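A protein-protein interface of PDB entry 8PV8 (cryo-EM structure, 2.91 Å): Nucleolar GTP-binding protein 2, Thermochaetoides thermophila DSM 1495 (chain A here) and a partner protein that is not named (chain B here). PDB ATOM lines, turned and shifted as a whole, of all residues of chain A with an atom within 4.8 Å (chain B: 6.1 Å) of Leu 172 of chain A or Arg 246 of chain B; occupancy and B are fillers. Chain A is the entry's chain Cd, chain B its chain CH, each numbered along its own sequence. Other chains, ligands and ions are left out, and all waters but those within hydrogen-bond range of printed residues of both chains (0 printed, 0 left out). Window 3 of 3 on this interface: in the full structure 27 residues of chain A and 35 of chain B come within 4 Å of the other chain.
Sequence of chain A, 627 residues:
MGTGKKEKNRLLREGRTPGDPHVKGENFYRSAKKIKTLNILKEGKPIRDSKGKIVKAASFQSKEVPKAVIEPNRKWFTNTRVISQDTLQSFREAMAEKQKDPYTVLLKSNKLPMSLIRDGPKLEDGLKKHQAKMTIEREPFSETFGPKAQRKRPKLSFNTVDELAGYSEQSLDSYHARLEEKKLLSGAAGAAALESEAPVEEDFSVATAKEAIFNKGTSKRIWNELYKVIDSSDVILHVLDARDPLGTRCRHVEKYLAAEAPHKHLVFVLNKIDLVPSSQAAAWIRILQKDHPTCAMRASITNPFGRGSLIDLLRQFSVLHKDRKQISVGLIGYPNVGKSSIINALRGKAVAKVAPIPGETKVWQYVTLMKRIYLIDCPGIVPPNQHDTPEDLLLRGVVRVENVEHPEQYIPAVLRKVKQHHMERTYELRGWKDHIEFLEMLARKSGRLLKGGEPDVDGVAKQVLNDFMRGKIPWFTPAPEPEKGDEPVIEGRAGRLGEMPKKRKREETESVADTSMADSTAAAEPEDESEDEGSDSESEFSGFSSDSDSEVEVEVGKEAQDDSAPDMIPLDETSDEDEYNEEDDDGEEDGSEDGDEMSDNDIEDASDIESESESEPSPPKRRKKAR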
ATOM      1  N   SER A 168      -1.020 -16.074   9.700  1.00  0.00           N
ATOM      2  CA  SER A 168       0.322 -16.281   9.164  1.00  0.00           C
ATOM      3  C   SER A 168       1.253 -15.142   9.560  1.00  0.00           C
ATOM      4  O   SER A 168       2.412 -15.373   9.925  1.00  0.00           O
ATOM      5  CB  SER A 168       0.263 -16.432   7.644  1.00  0.00           C
ATOM      6  OG  SER A 168      -0.388 -15.327   7.045  1.00  0.00           O
ATOM      7  N   GLU A 169       0.752 -13.902   9.512  1.00  0.00           N
ATOM      8  CA  GLU A 169       1.572 -12.752   9.887  1.00  0.00           C
ATOM      9  C   GLU A 169       1.945 -12.789  11.367  1.00  0.00           C
ATOM     10  O   GLU A 169       3.109 -12.569  11.733  1.00  0.00           O
ATOM     11  CB  GLU A 169       0.835 -11.456   9.546  1.00  0.00           C
ATOM     12  CG  GLU A 169       1.617 -10.185   9.852  1.00  0.00           C
ATOM     13  CD  GLU A 169       2.869 -10.031   9.002  1.00  0.00           C
ATOM     14  OE1 GLU A 169       2.914 -10.584   7.882  1.00  0.00           O
ATOM     15  OE2 GLU A 169       3.813  -9.353   9.459  1.00  0.00           O
ATOM     16  N   GLN A 170       0.968 -13.081  12.233  1.00  0.00           N
ATOM     17  CA  GLN A 170       1.240 -13.160  13.667  1.00  0.00           C
ATOM     18  C   GLN A 170       2.175 -14.316  13.998  1.00  0.00           C
ATOM     19  O   GLN A 170       3.056 -14.180  14.857  1.00  0.00           O
ATOM     20  CB  GLN A 170      -0.068 -13.294  14.447  1.00  0.00           C
ATOM     21  CG  GLN A 170      -0.962 -12.070  14.383  1.00  0.00           C
ATOM     22  CD  GLN A 170      -2.253 -12.255  15.152  1.00  0.00           C
ATOM     23  OE1 GLN A 170      -2.521 -13.329  15.689  1.00  0.00           O
ATOM     24  NE2 GLN A 170      -3.064 -11.206  15.207  1.00  0.00           N
ATOM     25  N   SER A 171       2.002 -15.459  13.328  1.00  0.00           N
ATOM     26  CA  SER A 171       2.882 -16.599  13.556  1.00  0.00           C
ATOM     27  C   SER A 171       4.309 -16.292  13.125  1.00  0.00           C
ATOM     28  O   SER A 171       5.262 -16.665  13.816  1.00  0.00           O
ATOM     29  CB  SER A 171       2.353 -17.827  12.816  1.00  0.00           C
ATOM     30  OG  SER A 171       1.109 -18.245  13.348  1.00  0.00           O
ATOM     31  N   LEU A 172       4.474 -15.599  11.994  1.00  0.00           N
ATOM     32  CA  LEU A 172       5.809 -15.224  11.538  1.00  0.00           C
ATOM     33  C   LEU A 172       6.471 -14.238  12.496  1.00  0.00           C
ATOM     34  O   LEU A 172       7.670 -14.359  12.788  1.00  0.00           O
ATOM     35  CB  LEU A 172       5.728 -14.635  10.132  1.00  0.00           C
ATOM     36  CG  LEU A 172       7.055 -14.267   9.472  1.00  0.00           C
ATOM     37  CD1 LEU A 172       7.910 -15.506   9.275  1.00  0.00           C
ATOM     38  CD2 LEU A 172       6.813 -13.560   8.149  1.00  0.00           C
ATOM     39  N   ASP A 173       5.707 -13.262  12.998  1.00  0.00           N
ATOM     40  CA  ASP A 173       6.260 -12.300  13.951  1.00  0.00           C
ATOM     41  C   ASP A 173       6.663 -12.979  15.257  1.00  0.00           C
ATOM     42  O   ASP A 173       7.737 -12.701  15.809  1.00  0.00           O
ATOM     43  CB  ASP A 173       5.252 -11.182  14.214  1.00  0.00           C
ATOM     44  CG  ASP A 173       4.947 -10.369  12.973  1.00  0.00           C
ATOM     45  OD1 ASP A 173       5.739 -10.436  12.009  1.00  0.00           O
ATOM     46  OD2 ASP A 173       3.915  -9.667  12.960  1.00  0.00           O
ATOM     47  N   SER A 174       5.819 -13.886  15.756  1.00  0.00           N
ATOM     48  CA  SER A 174       6.150 -14.619  16.974  1.00  0.00           C
ATOM     49  C   SER A 174       7.358 -15.524  16.766  1.00  0.00           C
ATOM     50  O   SER A 174       8.195 -15.668  17.665  1.00  0.00           O
ATOM     51  CB  SER A 174       4.941 -15.429  17.440  1.00  0.00           C
ATOM     52  OG  SER A 174       5.235 -16.147  18.625  1.00  0.00           O
ATOM     53  N   TYR A 175       7.466 -16.136  15.583  1.00  0.00           N
ATOM     54  CA  TYR A 175       8.611 -16.984  15.266  1.00  0.00           C
ATOM     55  C   TYR A 175       9.901 -16.173  15.263  1.00  0.00           C
ATOM     56  O   TYR A 175      10.912 -16.583  15.850  1.00  0.00           O
ATOM     57  CB  TYR A 175       8.367 -17.658  13.911  1.00  0.00           C
ATOM     58  CG  TYR A 175       9.525 -18.438  13.327  1.00  0.00           C
ATOM     59  CD1 TYR A 175       9.831 -19.716  13.783  1.00  0.00           C
ATOM     60  CD2 TYR A 175      10.304 -17.903  12.310  1.00  0.00           C
ATOM     61  CE1 TYR A 175      10.877 -20.439  13.237  1.00  0.00           C
ATOM     62  CE2 TYR A 175      11.358 -18.612  11.769  1.00  0.00           C
ATOM     63  CZ  TYR A 175      11.642 -19.875  12.238  1.00  0.00           C
ATOM     64  OH  TYR A 175      12.692 -20.577  11.694  1.00  0.00           O
ATOM     65  N   HIS A 176       9.873 -14.996  14.635  1.00  0.00           N
ATOM     66  CA  HIS A 176      11.060 -14.145  14.614  1.00  0.00           C
ATOM     67  C   HIS A 176      11.429 -13.671  16.014  1.00  0.00           C
ATOM     68  O   HIS A 176      12.614 -13.608  16.362  1.00  0.00           O
ATOM     69  CB  HIS A 176      10.841 -12.959  13.680  1.00  0.00           C
ATOM     70  CG  HIS A 176      10.900 -13.320  12.229  1.00  0.00           C
ATOM     71  ND1 HIS A 176      11.880 -14.133  11.702  1.00  0.00           N
ATOM     72  CD2 HIS A 176      10.096 -12.980  11.195  1.00  0.00           C
ATOM     73  CE1 HIS A 176      11.681 -14.272  10.404  1.00  0.00           C
ATOM     74  NE2 HIS A 176      10.604 -13.584  10.071  1.00  0.00           N
ATOM     75  N   HIS B  74       9.302 -23.305  11.804  1.00  0.00           N
ATOM     76  CA  HIS B  74       8.770 -22.204  11.018  1.00  0.00           C
ATOM     77  C   HIS B  74       7.257 -22.365  10.901  1.00  0.00           C
ATOM     78  O   HIS B  74       6.756 -23.496  10.931  1.00  0.00           O
ATOM     79  CB  HIS B  74       9.426 -22.184   9.635  1.00  0.00           C
ATOM     80  CG  HIS B  74       9.115 -20.962   8.829  1.00  0.00           C
ATOM     81  ND1 HIS B  74       7.988 -20.855   8.044  1.00  0.00           N
ATOM     82  CD2 HIS B  74       9.782 -19.792   8.690  1.00  0.00           C
ATOM     83  CE1 HIS B  74       7.974 -19.672   7.456  1.00  0.00           C
ATOM     84  NE2 HIS B  74       9.053 -19.008   7.830  1.00  0.00           N
ATOM     85  N   PRO B  75       6.497 -21.262  10.827  1.00  0.00           N
ATOM     86  CA  PRO B  75       5.031 -21.383  10.715  1.00  0.00           C
ATOM     87  C   PRO B  75       4.555 -22.191   9.518  1.00  0.00           C
ATOM     88  O   PRO B  75       3.522 -22.866   9.614  1.00  0.00           O
ATOM     89  CB  PRO B  75       4.579 -19.922  10.625  1.00  0.00           C
ATOM     90  CG  PRO B  75       5.597 -19.180  11.401  1.00  0.00           C
ATOM     91  CD  PRO B  75       6.905 -19.895  11.196  1.00  0.00           C
ATOM     92  N   ARG B  78       5.231 -25.848  10.710  1.00  0.00           N
ATOM     93  CA  ARG B  78       4.283 -26.166  11.773  1.00  0.00           C
ATOM     94  C   ARG B  78       2.876 -26.368  11.227  1.00  0.00           C
ATOM     95  O   ARG B  78       2.206 -27.354  11.556  1.00  0.00           O
ATOM     96  CB  ARG B  78       4.278 -25.051  12.819  1.00  0.00           C
ATOM     97  CG  ARG B  78       3.192 -25.196  13.872  1.00  0.00           C
ATOM     98  CD  ARG B  78       3.427 -24.258  15.037  1.00  0.00           C
ATOM     99  NE  ARG B  78       2.977 -22.905  14.740  1.00  0.00           N
ATOM    100  CZ  ARG B  78       3.728 -21.820  14.869  1.00  0.00           C
ATOM    101  NH1 ARG B  78       4.983 -21.893  15.281  1.00  0.00           N
ATOM    102  NH2 ARG B  78       3.208 -20.633  14.575  1.00  0.00           N
ATOM    103  N   PRO B 164      12.012 -22.260   3.954  1.00  0.00           N
ATOM    104  CA  PRO B 164      11.002 -21.189   4.017  1.00  0.00           C
ATOM    105  C   PRO B 164      11.516 -19.817   3.617  1.00  0.00           C
ATOM    106  O   PRO B 164      10.709 -18.967   3.219  1.00  0.00           O
ATOM    107  CB  PRO B 164      10.559 -21.208   5.487  1.00  0.00           C
ATOM    108  CG  PRO B 164      10.985 -22.542   6.009  1.00  0.00           C
ATOM    109  CD  PRO B 164      12.233 -22.885   5.268  1.00  0.00           C
ATOM    110  N   THR B 165      12.826 -19.564   3.705  1.00  0.00           N
ATOM    111  CA  THR B 165      13.403 -18.252   3.394  1.00  0.00           C
ATOM    112  C   THR B 165      14.473 -18.439   2.321  1.00  0.00           C
ATOM    113  O   THR B 165      15.661 -18.565   2.630  1.00  0.00           O
ATOM    114  CB  THR B 165      13.981 -17.587   4.651  1.00  0.00           C
ATOM    115  OG1 THR B 165      15.002 -18.423   5.209  1.00  0.00           O
ATOM    116  CG2 THR B 165      12.894 -17.350   5.692  1.00  0.00           C
ATOM    117  N   THR B 166      14.045 -18.432   1.059  1.00  0.00           N
ATOM    118  CA  THR B 166      14.941 -18.540  -0.084  1.00  0.00           C
ATOM    119  C   THR B 166      14.199 -18.056  -1.323  1.00  0.00           C
ATOM    120  O   THR B 166      13.040 -17.634  -1.253  1.00  0.00           O
ATOM    121  CB  THR B 166      15.444 -19.975  -0.276  1.00  0.00           C
ATOM    122  OG1 THR B 166      16.390 -20.013  -1.352  1.00  0.00           O
ATOM    123  CG2 THR B 166      14.290 -20.903  -0.598  1.00  0.00           C
ATOM    124  N   THR B 168      12.070 -18.715  -4.171  1.00  0.00           N
ATOM    125  CA  THR B 168      11.126 -19.799  -4.375  1.00  0.00           C
ATOM    126  C   THR B 168       9.952 -19.354  -5.242  1.00  0.00           C
ATOM    127  O   THR B 168       9.420 -18.246  -5.116  1.00  0.00           O
ATOM    128  CB  THR B 168      10.658 -20.378  -3.024  1.00  0.00           C
ATOM    129  OG1 THR B 168       9.851 -21.544  -3.238  1.00  0.00           O
ATOM    130  CG2 THR B 168       9.934 -19.358  -2.171  1.00  0.00           C
ATOM    131  N   ALA B 241       0.828 -23.592   1.772  1.00  0.00           N
ATOM    132  CA  ALA B 241       1.959 -23.127   0.975  1.00  0.00           C
ATOM    133  C   ALA B 241       1.723 -21.714   0.451  1.00  0.00           C
ATOM    134  O   ALA B 241       2.638 -20.882   0.450  1.00  0.00           O
ATOM    135  CB  ALA B 241       2.219 -24.095  -0.178  1.00  0.00           C
ATOM    136  N   ALA B 243      -0.187 -19.530   1.918  1.00  0.00           N
ATOM    137  CA  ALA B 243      -0.360 -18.621   3.043  1.00  0.00           C
ATOM    138  C   ALA B 243       0.952 -18.250   3.726  1.00  0.00           C
ATOM    139  O   ALA B 243       1.172 -17.074   4.031  1.00  0.00           O
ATOM    140  CB  ALA B 243      -1.313 -19.238   4.068  1.00  0.00           C
ATOM    141  N   HIS B 244       1.831 -19.220   3.974  1.00  0.00           N
ATOM    142  CA  HIS B 244       2.972 -18.991   4.850  1.00  0.00           C
ATOM    143  C   HIS B 244       4.306 -18.846   4.132  1.00  0.00           C
ATOM    144  O   HIS B 244       5.291 -18.466   4.774  1.00  0.00           O
ATOM    145  CB  HIS B 244       3.077 -20.126   5.876  1.00  0.00           C
ATOM    146  CG  HIS B 244       1.883 -20.232   6.770  1.00  0.00           C
ATOM    147  ND1 HIS B 244       0.716 -20.850   6.376  1.00  0.00           N
ATOM    148  CD2 HIS B 244       1.670 -19.795   8.033  1.00  0.00           C
ATOM    149  CE1 HIS B 244      -0.165 -20.786   7.357  1.00  0.00           C
ATOM    150  NE2 HIS B 244       0.390 -20.155   8.376  1.00  0.00           N
ATOM    151  N   LEU B 245       4.376 -19.127   2.836  1.00  0.00           N
ATOM    152  CA  LEU B 245       5.631 -19.071   2.099  1.00  0.00           C
ATOM    153  C   LEU B 245       5.707 -17.765   1.320  1.00  0.00           C
ATOM    154  O   LEU B 245       4.891 -17.526   0.424  1.00  0.00           O
ATOM    155  CB  LEU B 245       5.760 -20.261   1.152  1.00  0.00           C
ATOM    156  CG  LEU B 245       6.272 -21.563   1.760  1.00  0.00           C
ATOM    157  CD1 LEU B 245       6.092 -22.698   0.777  1.00  0.00           C
ATOM    158  CD2 LEU B 245       7.728 -21.423   2.153  1.00  0.00           C
ATOM    159  N   ARG B 246       6.688 -16.930   1.654  1.00  0.00           N
ATOM    160  CA  ARG B 246       6.968 -15.732   0.872  1.00  0.00           C
ATOM    161  C   ARG B 246       7.595 -16.174  -0.444  1.00  0.00           C
ATOM    162  O   ARG B 246       8.796 -16.455  -0.506  1.00  0.00           O
ATOM    163  CB  ARG B 246       7.887 -14.787   1.639  1.00  0.00           C
ATOM    164  CG  ARG B 246       8.135 -13.464   0.934  1.00  0.00           C
ATOM    165  CD  ARG B 246       9.027 -12.551   1.758  1.00  0.00           C
ATOM    166  NE  ARG B 246       8.399 -12.158   3.013  1.00  0.00           N
ATOM    167  CZ  ARG B 246       8.822 -12.532   4.213  1.00  0.00           C
ATOM    168  NH1 ARG B 246       9.882 -13.311   4.360  1.00  0.00           N
ATOM    169  NH2 ARG B 246       8.167 -12.112   5.291  1.00  0.00           N
ATOM    170  N   ALA B 247       6.787 -16.234  -1.495  1.00  0.00           N
ATOM    171  CA  ALA B 247       7.186 -16.892  -2.731  1.00  0.00           C
ATOM    172  C   ALA B 247       6.815 -15.995  -3.904  1.00  0.00           C
ATOM    173  O   ALA B 247       6.293 -14.887  -3.733  1.00  0.00           O
ATOM    174  CB  ALA B 247       6.527 -18.276  -2.828  1.00  0.00           C
ATOM    175  N   ALA B 248       7.093 -16.472  -5.113  1.00  0.00           N
ATOM    176  CA  ALA B 248       6.541 -15.902  -6.335  1.00  0.00           C
ATOM    177  C   ALA B 248       5.443 -16.847  -6.799  1.00  0.00           C
ATOM    178  O   ALA B 248       5.723 -17.972  -7.225  1.00  0.00           O
ATOM    179  CB  ALA B 248       7.615 -15.722  -7.404  1.00  0.00           C
ATOM    180  N   ASN B 279       2.095  -8.875  -0.168  1.00  0.00           N
ATOM    181  CA  ASN B 279       3.557  -8.904  -0.134  1.00  0.00           C
ATOM    182  C   ASN B 279       4.141 -10.073  -0.918  1.00  0.00           C
ATOM    183  O   ASN B 279       5.219 -10.573  -0.579  1.00  0.00           O
ATOM    184  CB  ASN B 279       4.094  -8.917   1.304  1.00  0.00           C
ATOM    185  CG  ASN B 279       3.740  -7.660   2.070  1.00  0.00           C
ATOM    186  OD1 ASN B 279       2.988  -7.703   3.043  1.00  0.00           O
ATOM    187  ND2 ASN B 279       4.285  -6.530   1.634  1.00  0.00           N
ATOM    188  N   LYS B 280       3.450 -10.523  -1.964  1.00  0.00           N
ATOM    189  CA  LYS B 280       3.924 -11.609  -2.808  1.00  0.00           C
ATOM    190  C   LYS B 280       3.773 -11.194  -4.262  1.00  0.00           C
ATOM    191  O   LYS B 280       2.917 -10.371  -4.596  1.00  0.00           O
ATOM    192  CB  LYS B 280       3.162 -12.915  -2.553  1.00  0.00           C
ATOM    193  CG  LYS B 280       3.197 -13.393  -1.114  1.00  0.00           C
ATOM    194  CD  LYS B 280       2.633 -14.790  -0.982  1.00  0.00           C
ATOM    195  CE  LYS B 280       2.589 -15.214   0.473  1.00  0.00           C
ATOM    196  NZ  LYS B 280       2.486 -16.689   0.609  1.00  0.00           N
ATOM    197  N   GLN B 345      14.898  -5.482  -1.580  1.00  0.00           N
ATOM    198  CA  GLN B 345      14.641  -5.653  -0.152  1.00  0.00           C
ATOM    199  C   GLN B 345      15.939  -5.747   0.645  1.00  0.00           C
ATOM    200  O   GLN B 345      16.019  -5.242   1.770  1.00  0.00           O
ATOM    201  CB  GLN B 345      13.776  -6.890   0.086  1.00  0.00           C
ATOM    202  CG  GLN B 345      12.329  -6.726  -0.343  1.00  0.00           C
ATOM    203  CD  GLN B 345      11.502  -7.970  -0.090  1.00  0.00           C
ATOM    204  OE1 GLN B 345      12.017  -8.993   0.359  1.00  0.00           O
ATOM    205  NE2 GLN B 345      10.208  -7.888  -0.379  1.00  0.00           N
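Of chain B, only His 74 (3.96 Å), Pro 75 (3.8 Å) and Arg 246 (3.5 Å) come within 4 Å of Leu 172 of chain A. Arg 246 of chain B touches just one residue of chain A: Leu 172 (3.5 Å). Of the printed residues of chain B, Tyr 175 of chain A touches His 74 (3.5 Å) and Pro 75 (3.7 Å). Of the printed residues of chain A, His 244 of chain B touches Ser 168. Printed residues of chain A within 4 Å of Arg 78 of chain B: Ser 171 (3.4 Å). Of the printed residues of chain B, Ser 171 of chain A touches Pro 75 (3.5 Å) and Arg 78 (3.4 Å). Of the printed residues of chain A, Ala 243 of chain B touches Ser 168. Ala 241 of chain B touches none of the printed residues of chain A. The nearest printed residue of chain A that does not touch Arg 246 of chain B is His 176 of chain A (5.6 Å).
Among the printed residues, merely in contact across the chains: Leu 172 of chain A with Arg 246 of chain B, Ser 171 of chain A with Pro 75 of chain B, Tyr 175 of chain A with His 74 of chain B, Ser 168 of chain A with His 244 of chain B, Tyr 175 of chain A with Pro 75 of chain B, Ser 168 of chain A with Ala 243 of chain B, Leu 172 of chain A with Pro 75 of chain B and Leu 172 of chain A with His 74 of chain B.
Of the 9 printed residues of chain A, 4 touch a printed residue of chain B. Hydrophobic or aromatic side chains of chain A that line the printed part of chain B: Leu 172 and Tyr 175. Of the 17 printed residues of chain B, 6 touch a printed residue of chain A. Hydrophobic or aromatic side chains of chain B within 4 Å of the printed part of chain A: His 74, Pro 75 and His 244. Along chain B the printed residues that touch a printed residue of chain A span positions 74 to 246.
The guanidinium group (NH2) of Arg 78 of chain B lies within hydrogen-bond range of the side-chain hydroxyl (OG) of Ser 171 of chain A, at 3.4 Å.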
